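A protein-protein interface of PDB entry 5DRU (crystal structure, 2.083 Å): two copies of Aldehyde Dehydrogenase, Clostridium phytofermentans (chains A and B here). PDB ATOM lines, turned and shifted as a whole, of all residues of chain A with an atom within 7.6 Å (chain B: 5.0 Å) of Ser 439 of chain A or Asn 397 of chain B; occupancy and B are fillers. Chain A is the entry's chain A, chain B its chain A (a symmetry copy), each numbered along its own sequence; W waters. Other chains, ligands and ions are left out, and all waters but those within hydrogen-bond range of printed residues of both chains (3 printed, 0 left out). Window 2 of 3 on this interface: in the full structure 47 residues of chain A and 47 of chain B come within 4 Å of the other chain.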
ATOM      1  N   GLY A  98     -33.863   8.284  26.689  1.00  0.00           N
ATOM      2  CA  GLY A  98     -34.103   9.497  25.923  1.00  0.00           C
ATOM      3  C   GLY A  98     -33.842   9.233  24.455  1.00  0.00           C
ATOM      4  O   GLY A  98     -33.910   8.083  24.018  1.00  0.00           O
ATOM      5  N   ASP A  99     -33.547  10.273  23.678  1.00  0.00           N
ATOM      6  CA  ASP A  99     -33.381  10.089  22.251  1.00  0.00           C
ATOM      7  C   ASP A  99     -32.252   9.106  21.953  1.00  0.00           C
ATOM      8  O   ASP A  99     -32.322   8.332  20.993  1.00  0.00           O
ATOM      9  CB  ASP A  99     -33.097  11.422  21.569  1.00  0.00           C
ATOM     10  CG  ASP A  99     -33.270  11.351  20.054  1.00  0.00           C
ATOM     11  OD1 ASP A  99     -32.355  11.781  19.318  1.00  0.00           O
ATOM     12  OD2 ASP A  99     -34.329  10.875  19.596  1.00  0.00           O
ATOM     13  N   ARG A 100     -31.220   9.134  22.783  1.00  0.00           N
ATOM     14  CA  ARG A 100     -30.056   8.317  22.531  1.00  0.00           C
ATOM     15  C   ARG A 100     -30.196   6.887  23.097  1.00  0.00           C
ATOM     16  O   ARG A 100     -29.235   6.084  23.090  1.00  0.00           O
ATOM     17  CB  ARG A 100     -28.832   9.046  23.072  1.00  0.00           C
ATOM     18  CG  ARG A 100     -28.664  10.415  22.387  1.00  0.00           C
ATOM     19  CD  ARG A 100     -27.516  11.248  22.941  1.00  0.00           C
ATOM     20  NE  ARG A 100     -27.052  12.233  21.960  1.00  0.00           N
ATOM     21  CZ  ARG A 100     -26.040  13.075  22.151  1.00  0.00           C
ATOM     22  NH1 ARG A 100     -25.368  13.076  23.293  1.00  0.00           N
ATOM     23  NH2 ARG A 100     -25.701  13.924  21.194  1.00  0.00           N
ATOM     24  N   GLY A 101     -31.395   6.531  23.563  1.00  0.00           N
ATOM     25  CA  GLY A 101     -31.650   5.138  23.939  1.00  0.00           C
ATOM     26  C   GLY A 101     -31.978   4.869  25.396  1.00  0.00           C
ATOM     27  O   GLY A 101     -32.647   5.637  26.079  1.00  0.00           O
ATOM     28  N   LEU A 102     -31.537   3.721  25.864  1.00  0.00           N
ATOM     29  CA  LEU A 102     -31.656   3.400  27.247  1.00  0.00           C
ATOM     30  C   LEU A 102     -30.324   3.079  27.882  1.00  0.00           C
ATOM     31  O   LEU A 102     -29.555   2.235  27.389  1.00  0.00           O
ATOM     32  CB  LEU A 102     -32.628   2.224  27.397  1.00  0.00           C
ATOM     33  CG  LEU A 102     -32.667   1.499  28.743  1.00  0.00           C
ATOM     34  CD1 LEU A 102     -33.411   2.306  29.801  1.00  0.00           C
ATOM     35  CD2 LEU A 102     -33.344   0.131  28.487  1.00  0.00           C
ATOM     36  N   THR A 103     -30.063   3.722  29.009  1.00  0.00           N
ATOM     37  CA  THR A 103     -28.884   3.359  29.850  1.00  0.00           C
ATOM     38  C   THR A 103     -29.315   2.779  31.194  1.00  0.00           C
ATOM     39  O   THR A 103     -30.089   3.381  31.907  1.00  0.00           O
ATOM     40  CB  THR A 103     -27.978   4.574  30.081  1.00  0.00           C
ATOM     41  OG1 THR A 103     -27.385   4.935  28.844  1.00  0.00           O
ATOM     42  CG2 THR A 103     -26.836   4.278  31.095  1.00  0.00           C
ATOM     43  N   CYS A 436     -24.787  -0.028  31.343  1.00  0.00           N
ATOM     44  CA  CYS A 436     -25.157  -0.687  30.136  1.00  0.00           C
ATOM     45  C   CYS A 436     -25.808   0.314  29.235  1.00  0.00           C
ATOM     46  O   CYS A 436     -26.866   0.811  29.557  1.00  0.00           O
ATOM     47  CB  CYS A 436     -26.106  -1.824  30.445  1.00  0.00           C
ATOM     48  SG  CYS A 436     -25.993  -3.085  29.266  1.00  0.00           S
ATOM     49  N   VAL A 437     -25.202   0.611  28.088  1.00  0.00           N
ATOM     50  CA  VAL A 437     -25.745   1.682  27.276  1.00  0.00           C
ATOM     51  C   VAL A 437     -26.354   1.089  26.026  1.00  0.00           C
ATOM     52  O   VAL A 437     -25.606   0.649  25.146  1.00  0.00           O
ATOM     53  CB  VAL A 437     -24.662   2.721  26.844  1.00  0.00           C
ATOM     54  CG1 VAL A 437     -25.291   3.819  25.951  1.00  0.00           C
ATOM     55  CG2 VAL A 437     -23.921   3.306  28.037  1.00  0.00           C
ATOM     56  N   MET A 438     -27.691   1.086  25.949  1.00  0.00           N
ATOM     57  CA  MET A 438     -28.415   0.613  24.768  1.00  0.00           C
ATOM     58  C   MET A 438     -28.703   1.813  23.897  1.00  0.00           C
ATOM     59  O   MET A 438     -29.565   2.645  24.221  1.00  0.00           O
ATOM     60  CB  MET A 438     -29.726  -0.097  25.140  1.00  0.00           C
ATOM     61  CG  MET A 438     -30.445  -0.731  23.943  1.00  0.00           C
ATOM     62  SD  MET A 438     -29.830  -2.320  23.361  1.00  0.00           S
ATOM     63  CE  MET A 438     -30.276  -3.326  24.781  1.00  0.00           C
ATOM     64  N   SER A 439     -27.953   1.931  22.817  1.00  0.00           N
ATOM     65  CA  SER A 439     -27.953   3.155  22.075  1.00  0.00           C
ATOM     66  C   SER A 439     -29.068   3.147  21.053  1.00  0.00           C
ATOM     67  O   SER A 439     -29.207   2.209  20.241  1.00  0.00           O
ATOM     68  CB  SER A 439     -26.612   3.364  21.376  1.00  0.00           C
ATOM     69  OG  SER A 439     -26.729   4.410  20.439  1.00  0.00           O
ATOM     70  N   ASP A 440     -29.835   4.218  21.103  1.00  0.00           N
ATOM     71  CA  ASP A 440     -30.778   4.589  20.021  1.00  0.00           C
ATOM     72  C   ASP A 440     -31.890   3.543  19.877  1.00  0.00           C
ATOM     73  O   ASP A 440     -32.553   3.444  18.839  1.00  0.00           O
ATOM     74  CB  ASP A 440     -30.012   4.810  18.719  1.00  0.00           C
ATOM     75  CG  ASP A 440     -29.089   6.038  18.788  1.00  0.00           C
ATOM     76  OD1 ASP A 440     -29.216   6.808  19.770  1.00  0.00           O
ATOM     77  OD2 ASP A 440     -28.253   6.238  17.872  1.00  0.00           O
ATOM     78  N   SER A 441     -32.102   2.788  20.958  1.00  0.00           N
ATOM     79  CA  SER A 441     -33.242   1.875  21.067  1.00  0.00           C
ATOM     80  C   SER A 441     -33.692   1.725  22.514  1.00  0.00           C
ATOM     81  O   SER A 441     -32.904   1.901  23.443  1.00  0.00           O
ATOM     82  CB  SER A 441     -32.895   0.485  20.529  1.00  0.00           C
ATOM     83  OG  SER A 441     -32.175  -0.217  21.536  1.00  0.00           O
ATOM     84  N   LEU A 442     -34.966   1.361  22.660  1.00  0.00           N
ATOM     85  CA  LEU A 442     -35.601   0.951  23.912  1.00  0.00           C
ATOM     86  C   LEU A 442     -35.878   2.149  24.835  1.00  0.00           C
ATOM     87  O   LEU A 442     -35.976   2.014  26.078  1.00  0.00           O
ATOM     88  CB  LEU A 442     -34.769  -0.136  24.605  1.00  0.00           C
ATOM     89  CG  LEU A 442     -34.672  -1.501  23.874  1.00  0.00           C
ATOM     90  CD1 LEU A 442     -34.141  -2.491  24.860  1.00  0.00           C
ATOM     91  CD2 LEU A 442     -35.962  -2.054  23.259  1.00  0.00           C
ATOM     92  N   LYS B 235     -23.088   0.504   9.833  1.00  0.00           N
ATOM     93  CA  LYS B 235     -23.053   1.387  10.977  1.00  0.00           C
ATOM     94  C   LYS B 235     -22.074   0.824  12.021  1.00  0.00           C
ATOM     95  O   LYS B 235     -21.360   1.585  12.668  1.00  0.00           O
ATOM     96  CB  LYS B 235     -24.447   1.587  11.579  1.00  0.00           C
ATOM     97  CG  LYS B 235     -24.496   2.805  12.490  1.00  0.00           C
ATOM     98  CD  LYS B 235     -25.757   2.897  13.318  1.00  0.00           C
ATOM     99  CE  LYS B 235     -25.531   3.787  14.558  1.00  0.00           C
ATOM    100  NZ  LYS B 235     -25.086   3.036  15.786  1.00  0.00           N
ATOM    101  N   ASP B 239     -19.092   3.099  13.658  1.00  0.00           N
ATOM    102  CA  ASP B 239     -19.026   3.307  15.096  1.00  0.00           C
ATOM    103  C   ASP B 239     -17.729   2.799  15.692  1.00  0.00           C
ATOM    104  O   ASP B 239     -17.173   3.416  16.593  1.00  0.00           O
ATOM    105  CB  ASP B 239     -20.199   2.609  15.772  1.00  0.00           C
ATOM    106  CG  ASP B 239     -21.494   3.340  15.597  1.00  0.00           C
ATOM    107  OD1 ASP B 239     -21.465   4.502  15.150  1.00  0.00           O
ATOM    108  OD2 ASP B 239     -22.538   2.731  15.923  1.00  0.00           O
ATOM    109  N   ILE B 374     -20.729  -4.266  22.088  1.00  0.00           N
ATOM    110  CA  ILE B 374     -21.374  -5.181  21.166  1.00  0.00           C
ATOM    111  C   ILE B 374     -22.194  -4.438  20.134  1.00  0.00           C
ATOM    112  O   ILE B 374     -22.868  -3.446  20.423  1.00  0.00           O
ATOM    113  CB  ILE B 374     -22.282  -6.203  21.936  1.00  0.00           C
ATOM    114  CG1 ILE B 374     -22.991  -7.134  20.959  1.00  0.00           C
ATOM    115  CG2 ILE B 374     -23.253  -5.468  22.883  1.00  0.00           C
ATOM    116  CD1 ILE B 374     -23.399  -8.475  21.559  1.00  0.00           C
ATOM    117  N   HIS B 375     -22.144  -4.962  18.937  1.00  0.00           N
ATOM    118  CA  HIS B 375     -23.125  -4.655  17.918  1.00  0.00           C
ATOM    119  C   HIS B 375     -23.958  -5.894  17.604  1.00  0.00           C
ATOM    120  O   HIS B 375     -23.448  -6.848  17.009  1.00  0.00           O
ATOM    121  CB  HIS B 375     -22.426  -4.147  16.678  1.00  0.00           C
ATOM    122  CG  HIS B 375     -21.805  -2.803  16.861  1.00  0.00           C
ATOM    123  ND1 HIS B 375     -22.397  -1.646  16.396  1.00  0.00           N
ATOM    124  CD2 HIS B 375     -20.655  -2.420  17.481  1.00  0.00           C
ATOM    125  CE1 HIS B 375     -21.621  -0.610  16.699  1.00  0.00           C
ATOM    126  NE2 HIS B 375     -20.568  -1.052  17.371  1.00  0.00           N
ATOM    127  N   SER B 376     -25.230  -5.863  18.014  1.00  0.00           N
ATOM    128  CA  SER B 376     -26.194  -6.927  17.736  1.00  0.00           C
ATOM    129  C   SER B 376     -27.591  -6.341  17.906  1.00  0.00           C
ATOM    130  O   SER B 376     -27.773  -5.517  18.760  1.00  0.00           O
ATOM    131  CB  SER B 376     -25.968  -8.114  18.671  1.00  0.00           C
ATOM    132  OG  SER B 376     -27.142  -8.884  18.889  1.00  0.00           O
ATOM    133  N   LYS B 377     -28.563  -6.731  17.087  1.00  0.00           N
ATOM    134  CA  LYS B 377     -29.944  -6.261  17.298  1.00  0.00           C
ATOM    135  C   LYS B 377     -30.754  -7.263  18.112  1.00  0.00           C
ATOM    136  O   LYS B 377     -31.970  -7.097  18.295  1.00  0.00           O
ATOM    137  CB  LYS B 377     -30.633  -5.992  15.962  1.00  0.00           C
ATOM    138  CG  LYS B 377     -30.022  -4.859  15.128  1.00  0.00           C
ATOM    139  CD  LYS B 377     -29.955  -3.539  15.897  1.00  0.00           C
ATOM    140  CE  LYS B 377     -29.485  -2.392  15.026  1.00  0.00           C
ATOM    141  NZ  LYS B 377     -30.399  -2.187  13.875  1.00  0.00           N
ATOM    142  N   VAL B 395     -21.306  -1.041  25.964  1.00  0.00           N
ATOM    143  CA  VAL B 395     -22.017  -0.247  25.014  1.00  0.00           C
ATOM    144  C   VAL B 395     -22.559  -1.182  23.937  1.00  0.00           C
ATOM    145  O   VAL B 395     -21.836  -2.034  23.468  1.00  0.00           O
ATOM    146  CB  VAL B 395     -21.130   0.827  24.419  1.00  0.00           C
ATOM    147  CG1 VAL B 395     -21.918   1.654  23.367  1.00  0.00           C
ATOM    148  CG2 VAL B 395     -20.537   1.707  25.544  1.00  0.00           C
ATOM    149  N   LYS B 396     -23.834  -0.986  23.576  1.00  0.00           N
ATOM    150  CA  LYS B 396     -24.542  -1.755  22.540  1.00  0.00           C
ATOM    151  C   LYS B 396     -24.862  -0.877  21.348  1.00  0.00           C
ATOM    152  O   LYS B 396     -25.526   0.130  21.517  1.00  0.00           O
ATOM    153  CB  LYS B 396     -25.847  -2.324  23.075  1.00  0.00           C
ATOM    154  CG  LYS B 396     -25.664  -3.405  24.112  1.00  0.00           C
ATOM    155  CD  LYS B 396     -26.743  -3.366  25.202  1.00  0.00           C
ATOM    156  CE  LYS B 396     -26.445  -2.279  26.263  1.00  0.00           C
ATOM    157  NZ  LYS B 396     -27.449  -2.275  27.430  1.00  0.00           N
ATOM    158  N   ASN B 397     -24.376  -1.243  20.164  1.00  0.00           N
ATOM    159  CA  ASN B 397     -24.676  -0.522  18.948  1.00  0.00           C
ATOM    160  C   ASN B 397     -24.369   0.966  19.027  1.00  0.00           C
ATOM    161  O   ASN B 397     -25.176   1.759  18.579  1.00  0.00           O
ATOM    162  CB  ASN B 397     -26.157  -0.700  18.584  1.00  0.00           C
ATOM    163  CG  ASN B 397     -26.591  -2.152  18.592  1.00  0.00           C
ATOM    164  OD1 ASN B 397     -25.851  -3.014  18.165  1.00  0.00           O
ATOM    165  ND2 ASN B 397     -27.761  -2.429  19.122  1.00  0.00           N
ATOM    166  N   ALA B 398     -23.209   1.358  19.570  1.00  0.00           N
ATOM    167  CA  ALA B 398     -22.725   2.746  19.406  1.00  0.00           C
ATOM    168  C   ALA B 398     -21.247   2.661  19.567  1.00  0.00           C
ATOM    169  O   ALA B 398     -20.778   1.632  20.021  1.00  0.00           O
ATOM    170  CB  ALA B 398     -23.320   3.723  20.452  1.00  0.00           C
ATOM    171  N   PRO B 399     -20.521   3.753  19.251  1.00  0.00           N
ATOM    172  CA  PRO B 399     -19.120   3.858  19.647  1.00  0.00           C
ATOM    173  C   PRO B 399     -18.938   3.854  21.162  1.00  0.00           C
ATOM    174  O   PRO B 399     -19.800   4.296  21.919  1.00  0.00           O
ATOM    175  CB  PRO B 399     -18.682   5.212  19.073  1.00  0.00           C
ATOM    176  CG  PRO B 399     -19.761   5.669  18.177  1.00  0.00           C
ATOM    177  CD  PRO B 399     -21.010   5.017  18.674  1.00  0.00           C
ATOM    178  N   GLY B 407     -23.111  10.941  22.893  1.00  0.00           N
ATOM    179  CA  GLY B 407     -24.002  10.140  22.064  1.00  0.00           C
ATOM    180  C   GLY B 407     -24.643   8.958  22.778  1.00  0.00           C
ATOM    181  O   GLY B 407     -25.076   8.020  22.111  1.00  0.00           O
HETATM  182  O   HOH W   1     -25.964   4.966  18.027  1.00  0.00           O
HETATM  183  O   HOH W   2     -29.678  -0.415  20.237  1.00  0.00           O
HETATM  184  O   HOH W   3     -27.045   9.056  19.471  1.00  0.00           O
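Water W1 lies within hydrogen-bond range of the side-chain hydroxyl (OG) of Ser 439 of chain A (2.6 Å), the side-chain carboxylate (OD2) of Asp 440 of chain A (2.6 Å), the side-chain amino group (NZ) of Lys 235 of chain B (3.1 Å) and the backbone carbonyl oxygen (O) of Asn 397 of chain B (3.3 Å).
Water W2 lies within hydrogen-bond range of O of Ser 439 of chain A (2.7 Å), OG of Ser 441 of chain A (2.8 Å), ND2 of Asn 397 of chain B (3.0 Å) and SD of Met 438 of chain A (3.7 Å).
Water W3 bridges OD1 of Asp 440 of chain A (3.1 Å) and O of Gly 407 of chain B (3.5 Å).
Gly 101 of chain A touches none of the printed residues of chain B.
Printed residues of chain B within 4 Å of Val 437 of chain A: Val 395 and Lys 396.
Lys 377 of chain B touches none of the printed residues of chain A.
Of the printed residues of chain A, Val 395 of chain B touches Val 437.
Asn 397 of chain B touches just one residue of chain A: Ser 439 (3.5 Å).
The nearest residue of chain B that does not touch Ser 439 of chain A is Gly 407 of chain B (4.3 Å).
The nearest printed residue of chain B that does not touch Met 438 of chain A is Asn 397 of chain B (4.7 Å).
The side-chain sulfur (SG) of Cys 436 of chain A lies within hydrogen-bond range of the side-chain amino group (NZ) of Lys 396 of chain B.
N of Ser 439 of chain A lies within hydrogen-bond range of O of Lys 396 of chain B (3.3 Å).
NH1 of Arg 100 of chain A lies close to N of Gly 407 of chain B (3.1 Å).
The backbone carbonyl oxygen (O) of Val 437 of chain A is in hydrogen-bond range of the backbone NH (N) of Lys 396 of chain B.
Val 437 of chain A touches Val 395 of chain B.
Met 438 of chain A touches Lys 396 of chain B (CE to CD, 3.6 Å).
Ser 439 of chain A touches Asn 397 of chain B.
Ser 439 of chain A touches Ala 398 of chain B.
No position is printed for both chains.
Of the 13 printed residues of chain A, 5 touch a printed residue of chain B.
Hydrophobic or aromatic side chains of chain A within 4 Å of the printed part of chain B: Met 438.
Hydrophobic or aromatic side chains of chain B that line the printed part of chain A: Ala 398.
Among the printed residues, no Asp or Glu carboxylate lies within 4 Å of a Lys or Arg side-chain nitrogen of the other chain.
N of Ile 374 of chain B lies within hydrogen-bond range of O of Val 395 of chain B (2.8 Å).
The side-chain amino group (NZ) of Lys 235 of chain B sits at hydrogen-bond distance from the backbone carbonyl oxygen (O) of Asn 397 of chain B (3.1 Å).
The backbone carbonyl oxygen of Ile 374 of chain B sits at hydrogen-bond distance from the backbone NH of Asn 397 of chain B, 2.7 Å away.
The side-chain hydroxyl (OG) of Ser 441 of chain A sits close to the side-chain sulfur (SD) of Met 438 of chain A (3.6 Å).
O of Leu 102 of chain A sits at hydrogen-bond distance from N of Met 438 of chain A, 2.6 Å away.
The backbone NH (N) of Asp 440 of chain A is in hydrogen-bond range of the backbone carbonyl oxygen (O) of Arg 100 of chain A, 2.8 Å away.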
